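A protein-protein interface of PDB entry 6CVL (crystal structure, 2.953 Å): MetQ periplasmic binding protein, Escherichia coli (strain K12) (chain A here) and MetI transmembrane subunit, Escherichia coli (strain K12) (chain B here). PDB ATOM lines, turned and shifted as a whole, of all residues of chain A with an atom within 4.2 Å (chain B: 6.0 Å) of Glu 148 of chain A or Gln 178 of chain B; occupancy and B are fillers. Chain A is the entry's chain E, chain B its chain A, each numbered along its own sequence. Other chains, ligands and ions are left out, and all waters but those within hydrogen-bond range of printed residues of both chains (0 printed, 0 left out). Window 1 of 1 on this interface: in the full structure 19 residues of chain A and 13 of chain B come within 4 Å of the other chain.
The backbone carbonyl oxygen of Gln 178 of chain B is in hydrogen-bond range of the backbone NH of Gly 183 of chain B (3.3 Å). O of Val 147 of chain A sits at hydrogen-bond distance from N of Val 102 of chain A (3.0 Å). The backbone carbonyl oxygen (O) of Val 102 of chain A is in hydrogen-bond range of the backbone NH (N) of Leu 149 of chain A (3.5 Å). O of Leu 149 of chain A sits at hydrogen-bond distance from N of Asn 104 of chain A (2.7 Å).
Printed residues of chain B within 4 Å of Asn 104 of chain A: Gln 178. Printed residues of chain B within 4 Å of Leu 109 of chain A: Gln 178. Of the printed residues of chain B, Val 147 of chain A touches Gly 168 (3.99 Å). Of chain B, only Ala 166, Gln 178 and Tyr 179 come within 4 Å of Glu 148 of chain A. Printed residues of chain B within 4 Å of Leu 149 of chain A: Ala 166. Of the printed residues of chain A, Ala 166 of chain B touches Glu 148 (3.9 Å) and Leu 149 (3.4 Å). Gln 178 of chain B touches just these residues of chain A: Asn 104 (3.5 Å), Leu 109 (3.2 Å) and Glu 148 (2.7 Å). Tyr 181 of chain B touches none of the printed residues of chain A. The nearest residue of chain B that does not touch Glu 148 of chain A is Gln 174 of chain B (4.1 Å).
Among the printed residues, pairs that only touch across the chains: Leu 109 of chain A with Gln 178 of chain B, Leu 149 of chain A with Ala 166 of chain B, Glu 148 of chain A with Ala 166 of chain B, Glu 148 of chain A with Tyr 179 of chain B and Val 147 of chain A with Gly 168 of chain B.
Hydrophobic or aromatic side chains of chain B within 4 Å of the printed part of chain A: Tyr 179. Hydrophobic or aromatic side chains of chain A within 4 Å of the printed part of chain B: Leu 109, Val 147 and Leu 149.
The side-chain amide nitrogen (NE2) of Gln 178 of chain B lies within hydrogen-bond range of the backbone carbonyl oxygen (O) of Asn 104 of chain A, 3.5 Å away. NE2 of Gln 178 of chain B sits at hydrogen-bond distance from OE1 of Glu 148 of chain A, 2.7 Å away.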
ATOM      1  N   VAL A 102      -9.818   5.673  21.016  1.00  0.00           N
ATOM      2  CA  VAL A 102      -9.368   5.190  22.322  1.00  0.00           C
ATOM      3  C   VAL A 102      -8.168   4.281  22.127  1.00  0.00           C
ATOM      4  O   VAL A 102      -7.973   3.698  21.052  1.00  0.00           O
ATOM      5  CB  VAL A 102     -10.481   4.435  23.072  1.00  0.00           C
ATOM      6  CG1 VAL A 102     -11.745   5.268  23.114  1.00  0.00           C
ATOM      7  CG2 VAL A 102     -10.741   3.085  22.421  1.00  0.00           C
ATOM      8  N   ASN A 104      -6.000   1.113  21.933  1.00  0.00           N
ATOM      9  CA  ASN A 104      -6.348  -0.281  21.692  1.00  0.00           C
ATOM     10  C   ASN A 104      -5.886  -1.205  22.809  1.00  0.00           C
ATOM     11  O   ASN A 104      -6.322  -2.359  22.851  1.00  0.00           O
ATOM     12  CB  ASN A 104      -5.765  -0.755  20.355  1.00  0.00           C
ATOM     13  CG  ASN A 104      -4.251  -0.704  20.318  1.00  0.00           C
ATOM     14  OD1 ASN A 104      -3.594  -0.557  21.347  1.00  0.00           O
ATOM     15  ND2 ASN A 104      -3.688  -0.828  19.120  1.00  0.00           N
ATOM     16  N   LEU A 109      -8.152   0.775  27.047  1.00  0.00           N
ATOM     17  CA  LEU A 109      -9.383   0.490  26.316  1.00  0.00           C
ATOM     18  C   LEU A 109     -10.571   0.431  27.267  1.00  0.00           C
ATOM     19  O   LEU A 109     -11.562   1.156  27.105  1.00  0.00           O
ATOM     20  CB  LEU A 109      -9.230  -0.825  25.552  1.00  0.00           C
ATOM     21  CG  LEU A 109     -10.460  -1.437  24.885  1.00  0.00           C
ATOM     22  CD1 LEU A 109     -11.046  -0.490  23.859  1.00  0.00           C
ATOM     23  CD2 LEU A 109     -10.078  -2.763  24.245  1.00  0.00           C
ATOM     24  N   VAL A 134     -15.289  -3.433  23.402  1.00  0.00           N
ATOM     25  CA  VAL A 134     -16.336  -3.074  22.459  1.00  0.00           C
ATOM     26  C   VAL A 134     -17.423  -4.136  22.423  1.00  0.00           C
ATOM     27  O   VAL A 134     -18.552  -3.852  22.006  1.00  0.00           O
ATOM     28  CB  VAL A 134     -15.743  -2.850  21.055  1.00  0.00           C
ATOM     29  CG1 VAL A 134     -16.800  -2.285  20.117  1.00  0.00           C
ATOM     30  CG2 VAL A 134     -14.530  -1.924  21.124  1.00  0.00           C
ATOM     31  N   VAL A 147     -12.798   3.297  17.968  1.00  0.00           N
ATOM     32  CA  VAL A 147     -11.582   3.121  17.185  1.00  0.00           C
ATOM     33  C   VAL A 147     -10.458   2.731  18.131  1.00  0.00           C
ATOM     34  O   VAL A 147     -10.279   3.361  19.179  1.00  0.00           O
ATOM     35  CB  VAL A 147     -11.221   4.405  16.415  1.00  0.00           C
ATOM     36  CG1 VAL A 147     -10.176   4.112  15.350  1.00  0.00           C
ATOM     37  CG2 VAL A 147     -12.473   5.023  15.802  1.00  0.00           C
ATOM     38  N   GLU A 148      -9.700   1.703  17.760  1.00  0.00           N
ATOM     39  CA  GLU A 148      -8.636   1.161  18.602  1.00  0.00           C
ATOM     40  C   GLU A 148      -7.312   1.293  17.857  1.00  0.00           C
ATOM     41  O   GLU A 148      -7.014   0.508  16.951  1.00  0.00           O
ATOM     42  CB  GLU A 148      -8.930  -0.286  18.978  1.00  0.00           C
ATOM     43  CG  GLU A 148     -10.278  -0.464  19.658  1.00  0.00           C
ATOM     44  CD  GLU A 148     -10.273  -1.561  20.702  1.00  0.00           C
ATOM     45  OE1 GLU A 148      -9.200  -1.839  21.279  1.00  0.00           O
ATOM     46  OE2 GLU A 148     -11.347  -2.145  20.950  1.00  0.00           O
ATOM     47  N   LEU A 149      -6.523   2.285  18.252  1.00  0.00           N
ATOM     48  CA  LEU A 149      -5.222   2.562  17.674  1.00  0.00           C
ATOM     49  C   LEU A 149      -4.143   2.329  18.723  1.00  0.00           C
ATOM     50  O   LEU A 149      -4.427   2.043  19.890  1.00  0.00           O
ATOM     51  CB  LEU A 149      -5.136   4.006  17.169  1.00  0.00           C
ATOM     52  CG  LEU A 149      -6.300   4.649  16.418  1.00  0.00           C
ATOM     53  CD1 LEU A 149      -7.488   4.917  17.331  1.00  0.00           C
ATOM     54  CD2 LEU A 149      -5.820   5.947  15.778  1.00  0.00           C
ATOM     55  N   ALA B 166      -3.272  -1.273  12.344  1.00  0.00           N
ATOM     56  CA  ALA B 166      -3.744  -0.816  13.642  1.00  0.00           C
ATOM     57  C   ALA B 166      -3.854   0.700  13.732  1.00  0.00           C
ATOM     58  O   ALA B 166      -3.870   1.248  14.840  1.00  0.00           O
ATOM     59  CB  ALA B 166      -2.829  -1.345  14.746  1.00  0.00           C
ATOM     60  N   VAL B 167      -3.920   1.387  12.596  1.00  0.00           N
ATOM     61  CA  VAL B 167      -4.564   2.710  12.533  1.00  0.00           C
ATOM     62  C   VAL B 167      -6.006   2.437  12.110  1.00  0.00           C
ATOM     63  O   VAL B 167      -6.405   2.589  10.952  1.00  0.00           O
ATOM     64  CB  VAL B 167      -3.833   3.676  11.599  1.00  0.00           C
ATOM     65  CG1 VAL B 167      -2.400   3.850  12.054  1.00  0.00           C
ATOM     66  CG2 VAL B 167      -3.883   3.184  10.161  1.00  0.00           C
ATOM     67  N   GLY B 168      -6.815   2.030  13.082  1.00  0.00           N
ATOM     68  CA  GLY B 168      -8.209   1.757  12.806  1.00  0.00           C
ATOM     69  C   GLY B 168      -8.484   0.553  11.928  1.00  0.00           C
ATOM     70  O   GLY B 168      -9.627   0.368  11.498  1.00  0.00           O
ATOM     71  N   ALA B 169      -7.478  -0.262  11.637  1.00  0.00           N
ATOM     72  CA  ALA B 169      -7.647  -1.468  10.832  1.00  0.00           C
ATOM     73  C   ALA B 169      -6.806  -2.555  11.494  1.00  0.00           C
ATOM     74  O   ALA B 169      -6.399  -2.433  12.655  1.00  0.00           O
ATOM     75  CB  ALA B 169      -7.267  -1.215   9.362  1.00  0.00           C
ATOM     76  N   GLY B 173      -5.583 -10.481  11.839  1.00  0.00           N
ATOM     77  CA  GLY B 173      -4.408 -10.489  12.691  1.00  0.00           C
ATOM     78  C   GLY B 173      -4.588  -9.618  13.918  1.00  0.00           C
ATOM     79  O   GLY B 173      -4.245 -10.017  15.034  1.00  0.00           O
ATOM     80  N   GLN B 174      -5.118  -8.411  13.727  1.00  0.00           N
ATOM     81  CA  GLN B 174      -5.467  -7.570  14.863  1.00  0.00           C
ATOM     82  C   GLN B 174      -6.442  -8.288  15.787  1.00  0.00           C
ATOM     83  O   GLN B 174      -6.278  -8.279  17.013  1.00  0.00           O
ATOM     84  CB  GLN B 174      -6.060  -6.256  14.358  1.00  0.00           C
ATOM     85  CG  GLN B 174      -6.665  -5.353  15.421  1.00  0.00           C
ATOM     86  CD  GLN B 174      -5.619  -4.606  16.212  1.00  0.00           C
ATOM     87  OE1 GLN B 174      -4.462  -5.021  16.276  1.00  0.00           O
ATOM     88  NE2 GLN B 174      -6.017  -3.493  16.820  1.00  0.00           N
ATOM     89  N   ILE B 175      -7.470  -8.916  15.215  1.00  0.00           N
ATOM     90  CA  ILE B 175      -8.454  -9.613  16.038  1.00  0.00           C
ATOM     91  C   ILE B 175      -7.785 -10.704  16.865  1.00  0.00           C
ATOM     92  O   ILE B 175      -8.049 -10.852  18.064  1.00  0.00           O
ATOM     93  CB  ILE B 175      -9.583 -10.187  15.165  1.00  0.00           C
ATOM     94  CG1 ILE B 175     -10.464  -9.056  14.638  1.00  0.00           C
ATOM     95  CG2 ILE B 175     -10.389 -11.197  15.962  1.00  0.00           C
ATOM     96  CD1 ILE B 175     -11.460  -9.495  13.598  1.00  0.00           C
ATOM     97  N   GLY B 176      -6.929 -11.500  16.229  1.00  0.00           N
ATOM     98  CA  GLY B 176      -6.230 -12.548  16.951  1.00  0.00           C
ATOM     99  C   GLY B 176      -5.349 -12.002  18.055  1.00  0.00           C
ATOM    100  O   GLY B 176      -5.293 -12.564  19.151  1.00  0.00           O
ATOM    101  N   TYR B 177      -4.646 -10.903  17.783  1.00  0.00           N
ATOM    102  CA  TYR B 177      -3.798 -10.303  18.805  1.00  0.00           C
ATOM    103  C   TYR B 177      -4.623  -9.857  20.006  1.00  0.00           C
ATOM    104  O   TYR B 177      -4.288 -10.167  21.154  1.00  0.00           O
ATOM    105  CB  TYR B 177      -3.022  -9.123  18.219  1.00  0.00           C
ATOM    106  CG  TYR B 177      -2.051  -8.486  19.193  1.00  0.00           C
ATOM    107  CD1 TYR B 177      -1.077  -9.244  19.826  1.00  0.00           C
ATOM    108  CD2 TYR B 177      -2.111  -7.127  19.479  1.00  0.00           C
ATOM    109  CE1 TYR B 177      -0.188  -8.669  20.717  1.00  0.00           C
ATOM    110  CE2 TYR B 177      -1.225  -6.542  20.369  1.00  0.00           C
ATOM    111  CZ  TYR B 177      -0.265  -7.318  20.984  1.00  0.00           C
ATOM    112  OH  TYR B 177       0.619  -6.743  21.872  1.00  0.00           O
ATOM    113  N   GLN B 178      -5.720  -9.141  19.758  1.00  0.00           N
ATOM    114  CA  GLN B 178      -6.476  -8.551  20.856  1.00  0.00           C
ATOM    115  C   GLN B 178      -7.291  -9.600  21.605  1.00  0.00           C
ATOM    116  O   GLN B 178      -7.095  -9.813  22.806  1.00  0.00           O
ATOM    117  CB  GLN B 178      -7.390  -7.440  20.332  1.00  0.00           C
ATOM    118  CG  GLN B 178      -7.263  -6.147  21.114  1.00  0.00           C
ATOM    119  CD  GLN B 178      -8.351  -5.152  20.778  1.00  0.00           C
ATOM    120  OE1 GLN B 178      -8.720  -4.985  19.615  1.00  0.00           O
ATOM    121  NE2 GLN B 178      -8.877  -4.486  21.801  1.00  0.00           N
ATOM    122  N   TYR B 179      -8.209 -10.265  20.909  1.00  0.00           N
ATOM    123  CA  TYR B 179      -9.166 -11.149  21.562  1.00  0.00           C
ATOM    124  C   TYR B 179      -8.676 -12.585  21.662  1.00  0.00           C
ATOM    125  O   TYR B 179      -9.013 -13.277  22.629  1.00  0.00           O
ATOM    126  CB  TYR B 179     -10.495 -11.101  20.811  1.00  0.00           C
ATOM    127  CG  TYR B 179     -11.024  -9.694  20.658  1.00  0.00           C
ATOM    128  CD1 TYR B 179     -11.852  -9.136  21.621  1.00  0.00           C
ATOM    129  CD2 TYR B 179     -10.685  -8.920  19.557  1.00  0.00           C
ATOM    130  CE1 TYR B 179     -12.335  -7.850  21.489  1.00  0.00           C
ATOM    131  CE2 TYR B 179     -11.164  -7.631  19.417  1.00  0.00           C
ATOM    132  CZ  TYR B 179     -11.989  -7.102  20.387  1.00  0.00           C
ATOM    133  OH  TYR B 179     -12.472  -5.821  20.257  1.00  0.00           O
ATOM    134  N   GLY B 180      -7.893 -13.052  20.690  1.00  0.00           N
ATOM    135  CA  GLY B 180      -7.358 -14.399  20.776  1.00  0.00           C
ATOM    136  C   GLY B 180      -6.253 -14.531  21.808  1.00  0.00           C
ATOM    137  O   GLY B 180      -6.165 -15.544  22.507  1.00  0.00           O
ATOM    138  N   TYR B 181      -5.400 -13.514  21.920  1.00  0.00           N
ATOM    139  CA  TYR B 181      -4.191 -13.586  22.731  1.00  0.00           C
ATOM    140  C   TYR B 181      -4.227 -12.718  23.981  1.00  0.00           C
ATOM    141  O   TYR B 181      -4.016 -13.229  25.086  1.00  0.00           O
ATOM    142  CB  TYR B 181      -2.981 -13.198  21.870  1.00  0.00           C
ATOM    143  CG  TYR B 181      -1.746 -12.881  22.671  1.00  0.00           C
ATOM    144  CD1 TYR B 181      -1.103 -13.862  23.414  1.00  0.00           C
ATOM    145  CD2 TYR B 181      -1.220 -11.599  22.682  1.00  0.00           C
ATOM    146  CE1 TYR B 181       0.031 -13.571  24.148  1.00  0.00           C
ATOM    147  CE2 TYR B 181      -0.089 -11.298  23.410  1.00  0.00           C
ATOM    148  CZ  TYR B 181       0.533 -12.286  24.142  1.00  0.00           C
ATOM    149  OH  TYR B 181       1.664 -11.986  24.868  1.00  0.00           O
ATOM    150  N   ILE B 182      -4.508 -11.419  23.852  1.00  0.00           N
ATOM    151  CA  ILE B 182      -4.479 -10.550  25.026  1.00  0.00           C
ATOM    152  C   ILE B 182      -5.594 -10.898  25.999  1.00  0.00           C
ATOM    153  O   ILE B 182      -5.527 -10.525  27.176  1.00  0.00           O
ATOM    154  CB  ILE B 182      -4.529  -9.070  24.592  1.00  0.00           C
ATOM    155  CG1 ILE B 182      -3.182  -8.674  23.974  1.00  0.00           C
ATOM    156  CG2 ILE B 182      -4.915  -8.165  25.756  1.00  0.00           C
ATOM    157  CD1 ILE B 182      -3.157  -7.292  23.353  1.00  0.00           C
ATOM    158  N   GLY B 183      -6.607 -11.622  25.546  1.00  0.00           N
ATOM    159  CA  GLY B 183      -7.666 -12.089  26.414  1.00  0.00           C
ATOM    160  C   GLY B 183      -7.796 -13.569  26.143  1.00  0.00           C
ATOM    161  O   GLY B 183      -8.195 -13.946  25.039  1.00  0.00           O
